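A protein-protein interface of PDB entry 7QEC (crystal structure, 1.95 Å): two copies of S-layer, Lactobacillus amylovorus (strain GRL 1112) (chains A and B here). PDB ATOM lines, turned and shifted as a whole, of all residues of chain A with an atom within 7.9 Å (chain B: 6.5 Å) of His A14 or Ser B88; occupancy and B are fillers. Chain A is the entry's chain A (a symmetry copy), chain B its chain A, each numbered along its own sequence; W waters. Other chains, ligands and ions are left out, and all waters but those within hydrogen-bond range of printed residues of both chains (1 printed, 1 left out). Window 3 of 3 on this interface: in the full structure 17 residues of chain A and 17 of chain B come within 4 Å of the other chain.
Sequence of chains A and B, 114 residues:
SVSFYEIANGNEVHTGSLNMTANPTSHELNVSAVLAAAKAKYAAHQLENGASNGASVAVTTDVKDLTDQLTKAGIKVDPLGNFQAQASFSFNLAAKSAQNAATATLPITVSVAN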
ATOM      1  N   SER A   3      -9.967  23.617  22.999  1.00  0.00           N
ATOM      2  CA  SER A   3     -11.411  23.414  23.091  1.00  0.00           C
ATOM      3  C   SER A   3     -12.002  24.181  24.274  1.00  0.00           C
ATOM      4  O   SER A   3     -11.307  24.522  25.237  1.00  0.00           O
ATOM      5  CB  SER A   3     -11.760  21.920  23.201  1.00  0.00           C
ATOM      6  OG  SER A   3     -10.909  21.253  24.105  1.00  0.00           O
ATOM      7  N   PHE A   4     -13.310  24.443  24.182  1.00  0.00           N
ATOM      8  CA  PHE A   4     -14.090  25.154  25.191  1.00  0.00           C
ATOM      9  C   PHE A   4     -14.924  24.164  26.001  1.00  0.00           C
ATOM     10  O   PHE A   4     -15.282  23.094  25.510  1.00  0.00           O
ATOM     11  CB  PHE A   4     -15.031  26.186  24.538  1.00  0.00           C
ATOM     12  CG  PHE A   4     -14.337  27.422  24.025  1.00  0.00           C
ATOM     13  CD1 PHE A   4     -13.770  27.441  22.749  1.00  0.00           C
ATOM     14  CD2 PHE A   4     -14.275  28.567  24.795  1.00  0.00           C
ATOM     15  CE1 PHE A   4     -13.145  28.580  22.268  1.00  0.00           C
ATOM     16  CE2 PHE A   4     -13.651  29.717  24.313  1.00  0.00           C
ATOM     17  CZ  PHE A   4     -13.078  29.712  23.050  1.00  0.00           C
ATOM     18  N   TYR A   5     -15.274  24.553  27.236  1.00  0.00           N
ATOM     19  CA  TYR A   5     -16.093  23.705  28.099  1.00  0.00           C
ATOM     20  C   TYR A   5     -16.966  24.570  28.997  1.00  0.00           C
ATOM     21  O   TYR A   5     -16.675  25.743  29.239  1.00  0.00           O
ATOM     22  CB  TYR A   5     -15.228  22.734  28.952  1.00  0.00           C
ATOM     23  CG  TYR A   5     -14.290  23.401  29.949  1.00  0.00           C
ATOM     24  CD1 TYR A   5     -14.739  23.780  31.220  1.00  0.00           C
ATOM     25  CD2 TYR A   5     -12.964  23.648  29.629  1.00  0.00           C
ATOM     26  CE1 TYR A   5     -13.870  24.399  32.148  1.00  0.00           C
ATOM     27  CE2 TYR A   5     -12.105  24.270  30.536  1.00  0.00           C
ATOM     28  CZ  TYR A   5     -12.570  24.644  31.794  1.00  0.00           C
ATOM     29  OH  TYR A   5     -11.713  25.248  32.698  1.00  0.00           O
ATOM     30  N   ASN A  11     -18.401  19.723  30.789  1.00  0.00           N
ATOM     31  CA  ASN A  11     -18.709  19.207  29.448  1.00  0.00           C
ATOM     32  C   ASN A  11     -18.121  20.095  28.346  1.00  0.00           C
ATOM     33  O   ASN A  11     -18.299  21.313  28.355  1.00  0.00           O
ATOM     34  CB  ASN A  11     -20.224  19.113  29.217  1.00  0.00           C
ATOM     35  CG  ASN A  11     -20.911  18.133  30.128  1.00  0.00           C
ATOM     36  OD1 ASN A  11     -20.318  17.150  30.577  1.00  0.00           O
ATOM     37  ND2 ASN A  11     -22.192  18.377  30.383  1.00  0.00           N
ATOM     38  N   GLU A  12     -17.489  19.480  27.351  1.00  0.00           N
ATOM     39  CA  GLU A  12     -17.065  20.223  26.168  1.00  0.00           C
ATOM     40  C   GLU A  12     -18.272  20.749  25.385  1.00  0.00           C
ATOM     41  O   GLU A  12     -19.327  20.104  25.322  1.00  0.00           O
ATOM     42  CB  GLU A  12     -16.198  19.326  25.276  1.00  0.00           C
ATOM     43  CG  GLU A  12     -15.606  20.022  24.057  1.00  0.00           C
ATOM     44  CD  GLU A  12     -14.585  19.157  23.332  1.00  0.00           C
ATOM     45  OE1 GLU A  12     -13.812  18.432  24.007  1.00  0.00           O
ATOM     46  OE2 GLU A  12     -14.559  19.198  22.083  1.00  0.00           O
ATOM     47  N   VAL A  13     -18.118  21.944  24.795  1.00  0.00           N
ATOM     48  CA  VAL A  13     -19.159  22.598  24.008  1.00  0.00           C
ATOM     49  C   VAL A  13     -18.525  23.129  22.731  1.00  0.00           C
ATOM     50  O   VAL A  13     -17.331  23.433  22.700  1.00  0.00           O
ATOM     51  CB  VAL A  13     -19.853  23.762  24.773  1.00  0.00           C
ATOM     52  CG1 VAL A  13     -20.616  23.252  26.004  1.00  0.00           C
ATOM     53  CG2 VAL A  13     -18.839  24.831  25.166  1.00  0.00           C
ATOM     54  N   HIS A  14     -19.318  23.234  21.667  1.00  0.00           N
ATOM     55  CA  HIS A  14     -18.842  23.923  20.471  1.00  0.00           C
ATOM     56  C   HIS A  14     -19.723  25.100  20.062  1.00  0.00           C
ATOM     57  O   HIS A  14     -19.335  25.849  19.156  1.00  0.00           O
ATOM     58  CB  HIS A  14     -18.656  22.943  19.291  1.00  0.00           C
ATOM     59  CG  HIS A  14     -19.920  22.567  18.580  1.00  0.00           C
ATOM     60  ND1 HIS A  14     -20.849  21.700  19.116  1.00  0.00           N
ATOM     61  CD2 HIS A  14     -20.394  22.920  17.361  1.00  0.00           C
ATOM     62  CE1 HIS A  14     -21.852  21.549  18.266  1.00  0.00           C
ATOM     63  NE2 HIS A  14     -21.600  22.278  17.191  1.00  0.00           N
ATOM     64  N   THR A  15     -20.862  25.309  20.729  1.00  0.00           N
ATOM     65  CA  THR A  15     -21.617  26.558  20.696  1.00  0.00           C
ATOM     66  C   THR A  15     -22.018  26.919  22.131  1.00  0.00           C
ATOM     67  O   THR A  15     -22.032  26.056  23.018  1.00  0.00           O
ATOM     68  CB  THR A  15     -22.882  26.443  19.829  1.00  0.00           C
ATOM     69  OG1 THR A  15     -23.727  25.412  20.366  1.00  0.00           O
ATOM     70  CG2 THR A  15     -22.523  26.096  18.403  1.00  0.00           C
ATOM     71  N   GLY A  16     -22.337  28.204  22.376  1.00  0.00           N
ATOM     72  CA  GLY A  16     -22.772  28.635  23.692  1.00  0.00           C
ATOM     73  C   GLY A  16     -24.101  29.389  23.632  1.00  0.00           C
ATOM     74  O   GLY A  16     -24.561  29.785  22.556  1.00  0.00           O
ATOM     75  N   TYR A  42     -18.335  29.755  30.587  1.00  0.00           N
ATOM     76  CA  TYR A  42     -17.495  29.013  29.643  1.00  0.00           C
ATOM     77  C   TYR A  42     -16.019  29.359  29.850  1.00  0.00           C
ATOM     78  O   TYR A  42     -15.675  30.500  30.173  1.00  0.00           O
ATOM     79  CB  TYR A  42     -17.897  29.318  28.171  1.00  0.00           C
ATOM     80  CG  TYR A  42     -19.345  28.981  27.824  1.00  0.00           C
ATOM     81  CD1 TYR A  42     -19.787  27.653  27.788  1.00  0.00           C
ATOM     82  CD2 TYR A  42     -20.255  29.980  27.535  1.00  0.00           C
ATOM     83  CE1 TYR A  42     -21.099  27.334  27.475  1.00  0.00           C
ATOM     84  CE2 TYR A  42     -21.587  29.671  27.218  1.00  0.00           C
ATOM     85  CZ  TYR A  42     -21.999  28.350  27.182  1.00  0.00           C
ATOM     86  OH  TYR A  42     -23.309  28.041  26.847  1.00  0.00           O
ATOM     87  N   ASN A  92     -18.731  36.326  19.354  1.00  0.00           N
ATOM     88  CA  ASN A  92     -17.727  35.258  19.466  1.00  0.00           C
ATOM     89  C   ASN A  92     -16.757  35.514  20.622  1.00  0.00           C
ATOM     90  O   ASN A  92     -16.233  36.628  20.774  1.00  0.00           O
ATOM     91  CB  ASN A  92     -16.920  35.108  18.166  1.00  0.00           C
ATOM     92  CG  ASN A  92     -17.783  34.741  16.952  1.00  0.00           C
ATOM     93  OD1 ASN A  92     -17.992  35.558  16.058  1.00  0.00           O
ATOM     94  ND2 ASN A  92     -18.255  33.511  16.906  1.00  0.00           N
ATOM     95  N   LEU A  93     -16.511  34.480  21.426  1.00  0.00           N
ATOM     96  CA  LEU A  93     -15.394  34.451  22.368  1.00  0.00           C
ATOM     97  C   LEU A  93     -14.170  33.854  21.686  1.00  0.00           C
ATOM     98  O   LEU A  93     -14.286  32.858  20.970  1.00  0.00           O
ATOM     99  CB  LEU A  93     -15.729  33.600  23.592  1.00  0.00           C
ATOM    100  CG  LEU A  93     -16.593  34.160  24.707  1.00  0.00           C
ATOM    101  CD1 LEU A  93     -16.617  33.132  25.833  1.00  0.00           C
ATOM    102  CD2 LEU A  93     -16.053  35.493  25.201  1.00  0.00           C
ATOM    103  N   ALA A 104      -9.002  29.589  18.575  1.00  0.00           N
ATOM    104  CA  ALA A 104     -10.314  28.956  18.528  1.00  0.00           C
ATOM    105  C   ALA A 104     -11.369  29.977  18.938  1.00  0.00           C
ATOM    106  O   ALA A 104     -11.090  30.902  19.705  1.00  0.00           O
ATOM    107  CB  ALA A 104     -10.375  27.726  19.438  1.00  0.00           C
ATOM    108  N   THR A 105     -12.581  29.810  18.413  1.00  0.00           N
ATOM    109  CA  THR A 105     -13.670  30.718  18.733  1.00  0.00           C
ATOM    110  C   THR A 105     -14.871  29.916  19.213  1.00  0.00           C
ATOM    111  O   THR A 105     -15.086  28.774  18.796  1.00  0.00           O
ATOM    112  CB  THR A 105     -14.053  31.642  17.516  1.00  0.00           C
ATOM    113  OG1 THR A 105     -14.355  30.855  16.358  1.00  0.00           O
ATOM    114  CG2 THR A 105     -12.916  32.601  17.179  1.00  0.00           C
ATOM    115  N   LEU A 106     -15.631  30.518  20.126  1.00  0.00           N
ATOM    116  CA  LEU A 106     -16.892  29.950  20.612  1.00  0.00           C
ATOM    117  C   LEU A 106     -18.023  30.914  20.281  1.00  0.00           C
ATOM    118  O   LEU A 106     -18.053  32.028  20.839  1.00  0.00           O
ATOM    119  CB  LEU A 106     -16.839  29.712  22.125  1.00  0.00           C
ATOM    120  CG  LEU A 106     -18.102  29.087  22.737  1.00  0.00           C
ATOM    121  CD1 LEU A 106     -18.316  27.672  22.181  1.00  0.00           C
ATOM    122  CD2 LEU A 106     -18.040  29.059  24.302  1.00  0.00           C
ATOM    123  N   PRO A 107     -18.954  30.556  19.394  1.00  0.00           N
ATOM    124  CA  PRO A 107     -20.096  31.446  19.101  1.00  0.00           C
ATOM    125  C   PRO A 107     -21.156  31.335  20.188  1.00  0.00           C
ATOM    126  O   PRO A 107     -21.564  30.231  20.557  1.00  0.00           O
ATOM    127  CB  PRO A 107     -20.628  30.918  17.761  1.00  0.00           C
ATOM    128  CG  PRO A 107     -20.287  29.431  17.788  1.00  0.00           C
ATOM    129  CD  PRO A 107     -18.979  29.323  18.580  1.00  0.00           C
ATOM    130  N   ILE A 108     -21.626  32.484  20.674  1.00  0.00           N
ATOM    131  CA  ILE A 108     -22.594  32.535  21.769  1.00  0.00           C
ATOM    132  C   ILE A 108     -23.833  33.301  21.299  1.00  0.00           C
ATOM    133  O   ILE A 108     -23.728  34.454  20.883  1.00  0.00           O
ATOM    134  CB  ILE A 108     -21.986  33.177  23.024  1.00  0.00           C
ATOM    135  CG1 ILE A 108     -20.922  32.226  23.614  1.00  0.00           C
ATOM    136  CG2 ILE A 108     -23.080  33.466  24.079  1.00  0.00           C
ATOM    137  CD1 ILE A 108     -20.230  32.757  24.814  1.00  0.00           C
ATOM    138  N   ALA B  85     -10.710  28.558   8.144  1.00  0.00           N
ATOM    139  CA  ALA B  85     -12.024  28.341   8.728  1.00  0.00           C
ATOM    140  C   ALA B  85     -11.933  27.705  10.114  1.00  0.00           C
ATOM    141  O   ALA B  85     -11.039  26.907  10.407  1.00  0.00           O
ATOM    142  CB  ALA B  85     -12.883  27.477   7.800  1.00  0.00           C
ATOM    143  N   GLN B  86     -12.873  28.084  10.971  1.00  0.00           N
ATOM    144  CA  GLN B  86     -13.107  27.419  12.242  1.00  0.00           C
ATOM    145  C   GLN B  86     -14.206  26.377  12.071  1.00  0.00           C
ATOM    146  O   GLN B  86     -15.042  26.467  11.169  1.00  0.00           O
ATOM    147  CB  GLN B  86     -13.520  28.428  13.321  1.00  0.00           C
ATOM    148  CG  GLN B  86     -12.705  29.709  13.331  1.00  0.00           C
ATOM    149  CD  GLN B  86     -11.463  29.574  14.193  1.00  0.00           C
ATOM    150  OE1 GLN B  86     -11.481  28.887  15.213  1.00  0.00           O
ATOM    151  NE2 GLN B  86     -10.376  30.216  13.778  1.00  0.00           N
ATOM    152  N   ALA B  87     -14.207  25.387  12.964  1.00  0.00           N
ATOM    153  CA  ALA B  87     -15.313  24.435  12.994  1.00  0.00           C
ATOM    154  C   ALA B  87     -16.652  25.123  13.281  1.00  0.00           C
ATOM    155  O   ALA B  87     -17.684  24.736  12.718  1.00  0.00           O
ATOM    156  CB  ALA B  87     -15.037  23.348  14.033  1.00  0.00           C
ATOM    157  N   SER B  88     -16.664  26.121  14.174  1.00  0.00           N
ATOM    158  CA  SER B  88     -17.883  26.842  14.558  1.00  0.00           C
ATOM    159  C   SER B  88     -17.577  28.317  14.778  1.00  0.00           C
ATOM    160  O   SER B  88     -16.650  28.638  15.516  1.00  0.00           O
ATOM    161  CB  SER B  88     -18.496  26.272  15.848  1.00  0.00           C
ATOM    162  OG  SER B  88     -19.243  25.089  15.613  1.00  0.00           O
ATOM    163  N   PHE B  89     -18.363  29.214  14.166  1.00  0.00           N
ATOM    164  CA  PHE B  89     -18.252  30.646  14.448  1.00  0.00           C
ATOM    165  C   PHE B  89     -19.600  31.295  14.141  1.00  0.00           C
ATOM    166  O   PHE B  89     -20.499  30.648  13.604  1.00  0.00           O
ATOM    167  CB  PHE B  89     -17.103  31.304  13.658  1.00  0.00           C
ATOM    168  CG  PHE B  89     -17.319  31.355  12.149  1.00  0.00           C
ATOM    169  CD1 PHE B  89     -16.942  30.290  11.344  1.00  0.00           C
ATOM    170  CD2 PHE B  89     -17.863  32.484  11.545  1.00  0.00           C
ATOM    171  CE1 PHE B  89     -17.126  30.330   9.959  1.00  0.00           C
ATOM    172  CE2 PHE B  89     -18.062  32.533  10.171  1.00  0.00           C
ATOM    173  CZ  PHE B  89     -17.688  31.454   9.378  1.00  0.00           C
ATOM    174  N   SER B  90     -19.753  32.576  14.495  1.00  0.00           N
ATOM    175  CA  SER B  90     -21.044  33.244  14.285  1.00  0.00           C
ATOM    176  C   SER B  90     -20.857  34.672  13.781  1.00  0.00           C
ATOM    177  O   SER B  90     -19.764  35.232  13.825  1.00  0.00           O
ATOM    178  CB  SER B  90     -21.895  33.254  15.569  1.00  0.00           C
ATOM    179  OG  SER B  90     -21.302  34.054  16.588  1.00  0.00           O
ATOM    180  N   THR B 109     -25.240  31.054  13.281  1.00  0.00           N
ATOM    181  CA  THR B 109     -24.142  30.151  13.626  1.00  0.00           C
ATOM    182  C   THR B 109     -23.769  29.266  12.434  1.00  0.00           C
ATOM    183  O   THR B 109     -24.626  28.563  11.886  1.00  0.00           O
ATOM    184  CB  THR B 109     -24.522  29.270  14.820  1.00  0.00           C
ATOM    185  OG1 THR B 109     -24.830  30.097  15.951  1.00  0.00           O
ATOM    186  CG2 THR B 109     -23.363  28.352  15.190  1.00  0.00           C
ATOM    187  N   VAL B 110     -22.480  29.258  12.082  1.00  0.00           N
ATOM    188  CA  VAL B 110     -21.943  28.516  10.937  1.00  0.00           C
ATOM    189  C   VAL B 110     -21.183  27.288  11.430  1.00  0.00           C
ATOM    190  O   VAL B 110     -20.315  27.405  12.304  1.00  0.00           O
ATOM    191  CB  VAL B 110     -21.001  29.409  10.106  1.00  0.00           C
ATOM    192  CG1 VAL B 110     -20.520  28.682   8.833  1.00  0.00           C
ATOM    193  CG2 VAL B 110     -21.679  30.708   9.765  1.00  0.00           C
ATOM    194  N   SER B 111     -21.476  26.128  10.842  1.00  0.00           N
ATOM    195  CA  SER B 111     -20.704  24.905  11.038  1.00  0.00           C
ATOM    196  C   SER B 111     -19.973  24.553   9.746  1.00  0.00           C
ATOM    197  O   SER B 111     -20.587  24.537   8.674  1.00  0.00           O
ATOM    198  CB  SER B 111     -21.609  23.743  11.451  1.00  0.00           C
ATOM    199  OG  SER B 111     -21.958  23.828  12.822  1.00  0.00           O
ATOM    200  N   VAL B 112     -18.681  24.230   9.852  1.00  0.00           N
ATOM    201  CA  VAL B 112     -17.800  24.032   8.701  1.00  0.00           C
ATOM    202  C   VAL B 112     -17.306  22.588   8.669  1.00  0.00           C
ATOM    203  O   VAL B 112     -16.712  22.111   9.641  1.00  0.00           O
ATOM    204  CB  VAL B 112     -16.598  24.992   8.737  1.00  0.00           C
ATOM    205  CG1 VAL B 112     -15.695  24.747   7.536  1.00  0.00           C
ATOM    206  CG2 VAL B 112     -17.069  26.451   8.778  1.00  0.00           C
ATOM    207  N   ASN B 114     -14.808  21.630   6.994  1.00  0.00           N
ATOM    208  CA  ASN B 114     -13.341  21.715   6.912  1.00  0.00           C
ATOM    209  C   ASN B 114     -12.756  20.793   5.855  1.00  0.00           C
ATOM    210  O   ASN B 114     -11.550  20.845   5.627  1.00  0.00           O
ATOM    211  CB  ASN B 114     -12.684  21.413   8.259  1.00  0.00           C
ATOM    212  CG  ASN B 114     -12.193  22.662   8.961  1.00  0.00           C
ATOM    213  OD1 ASN B 114     -11.071  23.112   8.737  1.00  0.00           O
ATOM    214  ND2 ASN B 114     -13.026  23.221   9.829  1.00  0.00           N
ATOM    215  OXT ASN B 114     -13.459  20.010   5.207  1.00  0.00           O
HETATM  216  O   HOH W   1     -24.367  30.135  18.969  1.00  0.00           O
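The backbone carbonyl oxygen (O) of Ser B88 sits at hydrogen-bond distance from the side-chain hydroxyl (OG1) of Thr A105. OD1 of Asn A92 sits close to O of Ser B90 (2.9 Å).
O of Phe B89 sits at hydrogen-bond distance from N of Val B110 (2.9 Å). N of Gly A16 lies within hydrogen-bond range of O of Pro A107 (2.8 Å).
Among the printed residues, pairs that only touch across the chains: His A14 with Ser B88 (3.0 Å), Asn A92 with Phe B89 (3.8 Å), Ala A104 with Gln B86 (3.5 Å), Thr A105 with Gln B86 (3.5 Å), Thr A105 with Phe B89 (3.9 Å), Pro A107 with Ser B88 (3.9 Å), Pro A107 with Phe B89 (3.8 Å) and Pro A107 with Ser B90 (3.4 Å).
His A14 touches just one residue of chain B: Ser B88. Of chain A, only His A14, Thr A105 and Pro A107 come within 4 Å of Ser B88. Ala B87 touches none of the printed residues of chain A. Of the printed residues of chain B, Ala A104 touches Gln B86. Of the printed residues of chain B, Thr A105 touches Gln B86 (3.5 Å), Ser B88 (3.3 Å) and Phe B89 (3.9 Å).
Of the 11 printed residues of chain B, 4 touch a printed residue of chain A. Printed residues of chain B that touch a printed residue of chain A: Gln B86, Ser B88, Phe B89 and Ser B90. Printed residues of chain A that touch a printed residue of chain B: His A14, Asn A92, Ala A104, Thr A105 and Pro A107. Hydrophobic or aromatic side chains of chain A within 4 Å of the printed part of chain B: His A14 and Pro A107. Among the printed residues, 10 pairs touch across the chains. Among the printed residues, no Asp or Glu carboxylate lies within 4 Å of a Lys or Arg side-chain nitrogen of the other chain.
No position is printed for both chains. Of the 10 pairs that touch across the chains among the printed residues, none has its exchanged pair printed and touching as well.
Water W1 lies within hydrogen-bond range of the side-chain hydroxyl of Thr B109 (3.1 Å) and the backbone carbonyl oxygen of Pro A107 (3.2 Å).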
